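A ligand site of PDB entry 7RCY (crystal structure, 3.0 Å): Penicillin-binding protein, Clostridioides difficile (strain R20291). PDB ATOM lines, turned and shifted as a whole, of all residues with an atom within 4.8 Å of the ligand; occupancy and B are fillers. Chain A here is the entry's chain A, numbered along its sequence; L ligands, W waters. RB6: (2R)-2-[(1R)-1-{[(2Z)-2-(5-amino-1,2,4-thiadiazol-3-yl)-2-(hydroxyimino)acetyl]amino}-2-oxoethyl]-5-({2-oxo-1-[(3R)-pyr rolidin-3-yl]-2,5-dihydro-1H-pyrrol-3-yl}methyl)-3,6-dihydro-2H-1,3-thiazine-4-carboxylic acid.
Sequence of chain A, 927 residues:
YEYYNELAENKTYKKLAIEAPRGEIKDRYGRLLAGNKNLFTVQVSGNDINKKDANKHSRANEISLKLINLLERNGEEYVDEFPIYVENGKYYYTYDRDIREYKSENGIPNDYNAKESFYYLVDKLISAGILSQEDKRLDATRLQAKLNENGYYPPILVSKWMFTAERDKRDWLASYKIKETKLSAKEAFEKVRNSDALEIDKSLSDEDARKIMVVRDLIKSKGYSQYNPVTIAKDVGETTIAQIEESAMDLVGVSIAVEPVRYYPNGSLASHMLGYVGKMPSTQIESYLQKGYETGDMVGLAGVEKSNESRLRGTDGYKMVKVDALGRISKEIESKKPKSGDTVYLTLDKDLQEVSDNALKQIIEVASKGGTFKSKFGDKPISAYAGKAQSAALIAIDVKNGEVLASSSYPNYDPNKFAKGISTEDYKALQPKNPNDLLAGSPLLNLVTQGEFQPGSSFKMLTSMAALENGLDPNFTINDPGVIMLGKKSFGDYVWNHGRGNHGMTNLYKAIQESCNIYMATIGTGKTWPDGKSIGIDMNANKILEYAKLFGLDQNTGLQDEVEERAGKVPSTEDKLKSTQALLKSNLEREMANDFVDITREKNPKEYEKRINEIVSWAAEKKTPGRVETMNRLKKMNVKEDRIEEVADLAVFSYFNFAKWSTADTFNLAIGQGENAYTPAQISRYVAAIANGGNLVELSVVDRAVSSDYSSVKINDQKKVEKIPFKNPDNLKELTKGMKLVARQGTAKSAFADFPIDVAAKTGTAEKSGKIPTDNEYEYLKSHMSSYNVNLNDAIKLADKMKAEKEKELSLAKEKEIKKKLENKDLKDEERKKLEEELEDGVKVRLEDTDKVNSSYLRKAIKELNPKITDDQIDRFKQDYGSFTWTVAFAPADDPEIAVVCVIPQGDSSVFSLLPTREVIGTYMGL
Water W1 lies within hydrogen-bond range of NAN of the ligand (2.6 Å) and OG of Ser 909 (2.8 Å).
O of the ligand sits close to N of Ser 457, at 2.7 Å. OG of Ser 457 is covalently linked to C of the ligand. O of Thr 763 lies close to OBJ of the ligand. OG1 of Thr 763 is in hydrogen-bond range of OBJ of the ligand (3.3 Å). A nitrogen (NAC) of the ligand lies within hydrogen-bond range of the side-chain hydroxyl of Ser 515 (2.9 Å). OE1 of Gln 454 sits close to SBE of the ligand (3.0 Å). A nitrogen (NBF) of the ligand lies close to the side-chain amide nitrogen (NE2) of Gln 673 (3.1 Å). The backbone NH (N) of Thr 765 lies within hydrogen-bond range of an oxygen (O) of the ligand (3.5 Å). The backbone carbonyl oxygen (O) of Thr 765 is in hydrogen-bond range of a nitrogen (N) of the ligand. OG1 of Thr 765 lies within hydrogen-bond range of OBI of the ligand (3.1 Å). The side-chain amide nitrogen (ND2) of Asn 517 sits at hydrogen-bond distance from an oxygen (OAX) of the ligand (3.1 Å). The side-chain amino group (NZ) of Lys 762 lies within salt-bridge range of an oxygen (OBJ) of the ligand (3.3 Å).
The side-chain hydroxyl (OG) of Ser 457 sits at hydrogen-bond distance from the side-chain hydroxyl (OG) of Ser 515, 3.1 Å away. OG of Ser 457 lies within hydrogen-bond range of NZ of Lys 460 (3.3 Å). OG1 of Thr 747 lies within hydrogen-bond range of OG1 of Thr 763, at 2.4 Å. The backbone carbonyl oxygen of Ser 515 lies close to the side-chain amide oxygen of Asn 517, at 3.0 Å. The side-chain amino group of Lys 460 sits at hydrogen-bond distance from the side-chain hydroxyl of Ser 515 (2.7 Å). The backbone carbonyl oxygen (O) of Phe 884 lies within hydrogen-bond range of the backbone NH (N) of Ala 766, at 3.2 Å. The side-chain amide oxygen (OD1) of Asn 517 lies within hydrogen-bond range of the side-chain amino group (NZ) of Lys 460. The backbone carbonyl oxygen (O) of Gly 456 lies close to the backbone carbonyl oxygen (O) of Ile 671.
C of Gly 456 touches O of the ligand (3.4 Å). OH of Tyr 494 touches CAL of the ligand (3.0 Å). Ile 671 touches the ligand (CD1 to OAX, 3.4 Å). CA of Gly 764 touches O of the ligand, 3.9 Å away. Ala 766 touches the ligand (CB to NBC, 3.0 Å). Glu 767 touches the ligand (N to OBA, 3.9 Å). O of Asp 908 touches CAO of the ligand (3.3 Å). Hydrophobic or aromatic side chains that line the ligand: Tyr 494, Ile 671 and Ala 766. Of the 21 residues printed, 15 come within 4 Å of the ligand.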
ATOM      1  N   GLN A 454      14.606   6.659 -13.605  1.00  0.00           N
ATOM      2  CA  GLN A 454      14.907   5.477 -14.441  1.00  0.00           C
ATOM      3  C   GLN A 454      14.001   4.370 -13.949  1.00  0.00           C
ATOM      4  O   GLN A 454      14.114   4.011 -12.787  1.00  0.00           O
ATOM      5  CB  GLN A 454      16.321   5.017 -14.081  1.00  0.00           C
ATOM      6  CG  GLN A 454      17.365   5.238 -15.156  1.00  0.00           C
ATOM      7  CD  GLN A 454      18.626   4.477 -14.811  1.00  0.00           C
ATOM      8  OE1 GLN A 454      18.612   3.557 -14.004  1.00  0.00           O
ATOM      9  NE2 GLN A 454      19.726   4.864 -15.420  1.00  0.00           N
ATOM     10  N   GLY A 456      13.094   0.779 -13.106  1.00  0.00           N
ATOM     11  CA  GLY A 456      14.080  -0.287 -12.978  1.00  0.00           C
ATOM     12  C   GLY A 456      13.632  -1.553 -13.644  1.00  0.00           C
ATOM     13  O   GLY A 456      13.606  -1.632 -14.867  1.00  0.00           O
ATOM     14  N   SER A 457      13.216  -2.490 -12.819  1.00  0.00           N
ATOM     15  CA  SER A 457      12.820  -3.814 -13.305  1.00  0.00           C
ATOM     16  C   SER A 457      11.320  -3.856 -13.508  1.00  0.00           C
ATOM     17  O   SER A 457      10.802  -4.928 -13.730  1.00  0.00           O
ATOM     18  CB  SER A 457      13.250  -4.781 -12.308  1.00  0.00           C
ATOM     19  OG  SER A 457      14.611  -5.241 -12.555  1.00  0.00           O
ATOM     20  N   LYS A 460      10.428  -4.259 -17.387  1.00  0.00           N
ATOM     21  CA  LYS A 460      10.475  -5.661 -17.879  1.00  0.00           C
ATOM     22  C   LYS A 460       9.145  -6.140 -18.462  1.00  0.00           C
ATOM     23  O   LYS A 460       9.189  -6.921 -19.407  1.00  0.00           O
ATOM     24  CB  LYS A 460      10.975  -6.571 -16.755  1.00  0.00           C
ATOM     25  CG  LYS A 460      12.219  -6.071 -16.049  1.00  0.00           C
ATOM     26  CD  LYS A 460      13.346  -7.051 -16.085  1.00  0.00           C
ATOM     27  CE  LYS A 460      13.428  -7.873 -14.818  1.00  0.00           C
ATOM     28  NZ  LYS A 460      14.820  -7.997 -14.325  1.00  0.00           N
ATOM     29  N   TYR A 494      21.826  -9.561 -10.496  1.00  0.00           N
ATOM     30  CA  TYR A 494      22.357  -9.088  -9.191  1.00  0.00           C
ATOM     31  C   TYR A 494      22.854 -10.327  -8.432  1.00  0.00           C
ATOM     32  O   TYR A 494      23.903 -10.252  -7.759  1.00  0.00           O
ATOM     33  CB  TYR A 494      21.296  -8.296  -8.430  1.00  0.00           C
ATOM     34  CG  TYR A 494      21.551  -8.096  -6.961  1.00  0.00           C
ATOM     35  CD1 TYR A 494      22.297  -7.013  -6.497  1.00  0.00           C
ATOM     36  CD2 TYR A 494      21.041  -8.984  -6.036  1.00  0.00           C
ATOM     37  CE1 TYR A 494      22.533  -6.824  -5.150  1.00  0.00           C
ATOM     38  CE2 TYR A 494      21.261  -8.812  -4.683  1.00  0.00           C
ATOM     39  CZ  TYR A 494      22.000  -7.730  -4.235  1.00  0.00           C
ATOM     40  OH  TYR A 494      22.224  -7.568  -2.901  1.00  0.00           O
ATOM     41  N   SER A 515      13.104 -11.723 -11.309  1.00  0.00           N
ATOM     42  CA  SER A 515      13.737 -10.573 -11.997  1.00  0.00           C
ATOM     43  C   SER A 515      15.069 -10.991 -12.623  1.00  0.00           C
ATOM     44  O   SER A 515      16.092 -10.404 -12.257  1.00  0.00           O
ATOM     45  CB  SER A 515      13.904  -9.417 -11.036  1.00  0.00           C
ATOM     46  OG  SER A 515      14.287  -8.235 -11.721  1.00  0.00           O
ATOM     47  N   ASN A 517      17.615 -10.650 -15.385  1.00  0.00           N
ATOM     48  CA  ASN A 517      17.981  -9.685 -16.450  1.00  0.00           C
ATOM     49  C   ASN A 517      18.518 -10.455 -17.655  1.00  0.00           C
ATOM     50  O   ASN A 517      18.420  -9.963 -18.778  1.00  0.00           O
ATOM     51  CB  ASN A 517      19.058  -8.713 -15.999  1.00  0.00           C
ATOM     52  CG  ASN A 517      18.826  -8.227 -14.589  1.00  0.00           C
ATOM     53  OD1 ASN A 517      18.066  -8.843 -13.852  1.00  0.00           O
ATOM     54  ND2 ASN A 517      19.464  -7.129 -14.215  1.00  0.00           N
ATOM     55  N   ILE A 671      15.908  -3.854 -19.313  1.00  0.00           N
ATOM     56  CA  ILE A 671      15.809  -4.149 -17.855  1.00  0.00           C
ATOM     57  C   ILE A 671      15.607  -2.869 -17.033  1.00  0.00           C
ATOM     58  O   ILE A 671      15.809  -2.947 -15.795  1.00  0.00           O
ATOM     59  CB  ILE A 671      17.031  -4.959 -17.378  1.00  0.00           C
ATOM     60  CG1 ILE A 671      18.322  -4.135 -17.430  1.00  0.00           C
ATOM     61  CG2 ILE A 671      17.178  -6.244 -18.161  1.00  0.00           C
ATOM     62  CD1 ILE A 671      19.344  -4.577 -16.411  1.00  0.00           C
ATOM     63  N   GLN A 673      17.136   0.306 -17.217  1.00  0.00           N
ATOM     64  CA  GLN A 673      18.234   1.281 -17.443  1.00  0.00           C
ATOM     65  C   GLN A 673      18.071   1.872 -18.852  1.00  0.00           C
ATOM     66  O   GLN A 673      17.773   1.110 -19.778  1.00  0.00           O
ATOM     67  CB  GLN A 673      19.614   0.638 -17.274  1.00  0.00           C
ATOM     68  CG  GLN A 673      19.735  -0.256 -16.044  1.00  0.00           C
ATOM     69  CD  GLN A 673      21.144  -0.502 -15.553  1.00  0.00           C
ATOM     70  OE1 GLN A 673      22.094   0.209 -15.896  1.00  0.00           O
ATOM     71  NE2 GLN A 673      21.290  -1.538 -14.721  1.00  0.00           N
ATOM     72  N   THR A 747      10.275 -11.561  -5.730  1.00  0.00           N
ATOM     73  CA  THR A 747      11.050 -10.436  -5.155  1.00  0.00           C
ATOM     74  C   THR A 747      10.229  -9.683  -4.116  1.00  0.00           C
ATOM     75  O   THR A 747      10.845  -8.889  -3.381  1.00  0.00           O
ATOM     76  CB  THR A 747      11.480  -9.428  -6.226  1.00  0.00           C
ATOM     77  OG1 THR A 747      10.322  -9.094  -7.001  1.00  0.00           O
ATOM     78  CG2 THR A 747      12.571  -9.959  -7.124  1.00  0.00           C
ATOM     79  N   LYS A 762       5.441  -5.885  -9.286  1.00  0.00           N
ATOM     80  CA  LYS A 762       6.830  -5.965  -9.795  1.00  0.00           C
ATOM     81  C   LYS A 762       7.676  -4.915  -9.084  1.00  0.00           C
ATOM     82  O   LYS A 762       7.207  -3.769  -8.959  1.00  0.00           O
ATOM     83  CB  LYS A 762       6.911  -5.723 -11.301  1.00  0.00           C
ATOM     84  CG  LYS A 762       8.322  -5.866 -11.859  1.00  0.00           C
ATOM     85  CD  LYS A 762       8.794  -7.302 -12.012  1.00  0.00           C
ATOM     86  CE  LYS A 762      10.310  -7.436 -12.093  1.00  0.00           C
ATOM     87  NZ  LYS A 762      10.950  -7.410 -10.753  1.00  0.00           N
ATOM     88  N   THR A 763       8.871  -5.322  -8.664  1.00  0.00           N
ATOM     89  CA  THR A 763       9.825  -4.507  -7.868  1.00  0.00           C
ATOM     90  C   THR A 763      10.890  -3.970  -8.831  1.00  0.00           C
ATOM     91  O   THR A 763      11.264  -4.679  -9.800  1.00  0.00           O
ATOM     92  CB  THR A 763      10.345  -5.295  -6.657  1.00  0.00           C
ATOM     93  OG1 THR A 763      10.522  -6.673  -6.993  1.00  0.00           O
ATOM     94  CG2 THR A 763       9.398  -5.249  -5.472  1.00  0.00           C
ATOM     95  N   GLY A 764      11.268  -2.707  -8.649  1.00  0.00           N
ATOM     96  CA  GLY A 764      12.421  -2.082  -9.309  1.00  0.00           C
ATOM     97  C   GLY A 764      13.395  -1.578  -8.259  1.00  0.00           C
ATOM     98  O   GLY A 764      12.918  -0.984  -7.236  1.00  0.00           O
ATOM     99  N   THR A 765      14.694  -1.869  -8.434  1.00  0.00           N
ATOM    100  CA  THR A 765      15.750  -1.509  -7.440  1.00  0.00           C
ATOM    101  C   THR A 765      17.098  -1.330  -8.132  1.00  0.00           C
ATOM    102  O   THR A 765      17.429  -2.161  -8.971  1.00  0.00           O
ATOM    103  CB  THR A 765      15.793  -2.533  -6.287  1.00  0.00           C
ATOM    104  OG1 THR A 765      14.485  -2.835  -5.815  1.00  0.00           O
ATOM    105  CG2 THR A 765      16.593  -2.016  -5.106  1.00  0.00           C
ATOM    106  N   ALA A 766      17.833  -0.278  -7.761  1.00  0.00           N
ATOM    107  CA  ALA A 766      19.165   0.090  -8.306  1.00  0.00           C
ATOM    108  C   ALA A 766      20.098   0.562  -7.178  1.00  0.00           C
ATOM    109  O   ALA A 766      19.639   1.350  -6.334  1.00  0.00           O
ATOM    110  CB  ALA A 766      19.038   1.145  -9.367  1.00  0.00           C
ATOM    111  N   GLU A 767      21.357   0.110  -7.186  1.00  0.00           N
ATOM    112  CA  GLU A 767      22.358   0.447  -6.128  1.00  0.00           C
ATOM    113  C   GLU A 767      23.060   1.764  -6.503  1.00  0.00           C
ATOM    114  O   GLU A 767      22.922   2.201  -7.670  1.00  0.00           O
ATOM    115  CB  GLU A 767      23.367  -0.683  -5.945  1.00  0.00           C
ATOM    116  CG  GLU A 767      22.853  -1.810  -5.067  1.00  0.00           C
ATOM    117  CD  GLU A 767      23.846  -2.950  -4.871  1.00  0.00           C
ATOM    118  OE1 GLU A 767      24.285  -3.555  -5.880  1.00  0.00           O
ATOM    119  OE2 GLU A 767      24.194  -3.231  -3.693  1.00  0.00           O
ATOM    120  N   GLY A 882      22.270   7.639  -7.166  1.00  0.00           N
ATOM    121  CA  GLY A 882      22.024   6.655  -8.246  1.00  0.00           C
ATOM    122  C   GLY A 882      21.264   5.428  -7.791  1.00  0.00           C
ATOM    123  O   GLY A 882      21.258   4.453  -8.559  1.00  0.00           O
ATOM    124  N   PHE A 884      17.488   3.727  -5.918  1.00  0.00           N
ATOM    125  CA  PHE A 884      16.017   3.863  -5.737  1.00  0.00           C
ATOM    126  C   PHE A 884      15.366   2.491  -5.539  1.00  0.00           C
ATOM    127  O   PHE A 884      15.982   1.482  -5.880  1.00  0.00           O
ATOM    128  CB  PHE A 884      15.394   4.590  -6.934  1.00  0.00           C
ATOM    129  CG  PHE A 884      15.770   4.088  -8.303  1.00  0.00           C
ATOM    130  CD1 PHE A 884      15.265   2.893  -8.796  1.00  0.00           C
ATOM    131  CD2 PHE A 884      16.587   4.839  -9.139  1.00  0.00           C
ATOM    132  CE1 PHE A 884      15.591   2.444 -10.069  1.00  0.00           C
ATOM    133  CE2 PHE A 884      16.907   4.407 -10.416  1.00  0.00           C
ATOM    134  CZ  PHE A 884      16.414   3.204 -10.883  1.00  0.00           C
ATOM    135  N   ASP A 908      17.307   1.783  -1.166  1.00  0.00           N
ATOM    136  CA  ASP A 908      17.983   0.559  -1.719  1.00  0.00           C
ATOM    137  C   ASP A 908      17.233  -0.740  -1.419  1.00  0.00           C
ATOM    138  O   ASP A 908      17.466  -1.696  -2.158  1.00  0.00           O
ATOM    139  CB  ASP A 908      19.355   0.299  -1.110  1.00  0.00           C
ATOM    140  CG  ASP A 908      20.472   1.141  -1.677  1.00  0.00           C
ATOM    141  OD1 ASP A 908      20.164   2.156  -2.333  1.00  0.00           O
ATOM    142  OD2 ASP A 908      21.638   0.777  -1.451  1.00  0.00           O
ATOM    143  N   SER A 909      16.461  -0.798  -0.326  1.00  0.00           N
ATOM    144  CA  SER A 909      15.665  -1.996   0.055  1.00  0.00           C
ATOM    145  C   SER A 909      14.241  -1.872  -0.506  1.00  0.00           C
ATOM    146  O   SER A 909      13.569  -0.903  -0.180  1.00  0.00           O
ATOM    147  CB  SER A 909      15.661  -2.217   1.532  1.00  0.00           C
ATOM    148  OG  SER A 909      15.391  -3.575   1.818  1.00  0.00           O
ATOM    149  N   SER A 910      13.792  -2.852  -1.291  1.00  0.00           N
ATOM    150  CA  SER A 910      12.424  -2.863  -1.887  1.00  0.00           C
ATOM    151  C   SER A 910      11.374  -2.911  -0.778  1.00  0.00           C
ATOM    152  O   SER A 910      10.204  -2.603  -1.062  1.00  0.00           O
ATOM    153  CB  SER A 910      12.236  -3.968  -2.885  1.00  0.00           C
ATOM    154  OG  SER A 910      12.463  -5.228  -2.303  1.00  0.00           O
HETATM  155  OAX RB6 L   1      19.599  -4.253 -13.023  1.00  0.00           O
HETATM  156  CAW RB6 L   1      19.163  -3.752 -12.025  1.00  0.00           C
HETATM  157  CAY RB6 L   1      20.052  -2.599 -11.602  1.00  0.00           C
HETATM  158  CBB RB6 L   1      19.759  -1.221 -12.127  1.00  0.00           C
HETATM  159  NBF RB6 L   1      18.789  -0.979 -12.992  1.00  0.00           N
HETATM  160  SBE RB6 L   1      18.724   0.664 -13.350  1.00  0.00           S
HETATM  161  CBD RB6 L   1      20.094   1.049 -12.249  1.00  0.00           C
HETATM  162  NBG RB6 L   1      20.601   2.316 -12.072  1.00  0.00           N
HETATM  163  NBC RB6 L   1      20.511  -0.084 -11.685  1.00  0.00           N
HETATM  164  NAZ RB6 L   1      21.043  -2.923 -10.828  1.00  0.00           N
HETATM  165  OBA RB6 L   1      21.840  -1.922 -10.454  1.00  0.00           O
HETATM  166  N   RB6 L   1      17.951  -4.159 -11.375  1.00  0.00           N
HETATM  167  CA  RB6 L   1      17.025  -5.210 -11.818  1.00  0.00           C
HETATM  168  C   RB6 L   1      15.636  -4.507 -11.985  1.00  0.00           C
HETATM  169  O   RB6 L   1      15.418  -3.434 -11.471  1.00  0.00           O
HETATM  170  CB  RB6 L   1      16.937  -6.454 -10.808  1.00  0.00           C
HETATM  171  SAS RB6 L   1      18.342  -6.338  -9.799  1.00  0.00           S
HETATM  172  CAR RB6 L   1      17.795  -7.397  -8.474  1.00  0.00           C
HETATM  173  NAC RB6 L   1      15.782  -6.510  -9.925  1.00  0.00           N
HETATM  174  CAD RB6 L   1      15.803  -6.185  -8.548  1.00  0.00           C
HETATM  175  CBH RB6 L   1      14.166  -6.072  -7.968  1.00  0.00           C
HETATM  176  OBI RB6 L   1      14.164  -5.778  -6.783  1.00  0.00           O
HETATM  177  OBJ RB6 L   1      13.286  -6.276  -8.767  1.00  0.00           O
HETATM  178  CAE RB6 L   1      16.832  -6.626  -7.698  1.00  0.00           C
HETATM  179  CAF RB6 L   1      17.696  -5.798  -6.734  1.00  0.00           C
HETATM  180  CAG RB6 L   1      17.893  -6.070  -5.218  1.00  0.00           C
HETATM  181  CAH RB6 L   1      18.820  -5.160  -4.482  1.00  0.00           C
HETATM  182  OAI RB6 L   1      19.604  -4.411  -5.030  1.00  0.00           O
HETATM  183  CAQ RB6 L   1      17.071  -6.489  -4.243  1.00  0.00           C
HETATM  184  CAP RB6 L   1      17.638  -6.247  -2.828  1.00  0.00           C
HETATM  185  NAJ RB6 L   1      18.686  -5.241  -3.079  1.00  0.00           N
HETATM  186  CAK RB6 L   1      19.490  -4.458  -2.123  1.00  0.00           C
HETATM  187  CAL RB6 L   1      20.692  -5.281  -1.730  1.00  0.00           C
HETATM  188  CAM RB6 L   1      20.071  -6.368  -0.857  1.00  0.00           C
HETATM  189  NAN RB6 L   1      19.152  -5.612   0.007  1.00  0.00           N
HETATM  190  CAO RB6 L   1      18.910  -4.332  -0.686  1.00  0.00           C
HETATM  191  O   HOH W   1      17.101  -5.817   1.516  1.00  0.00           O
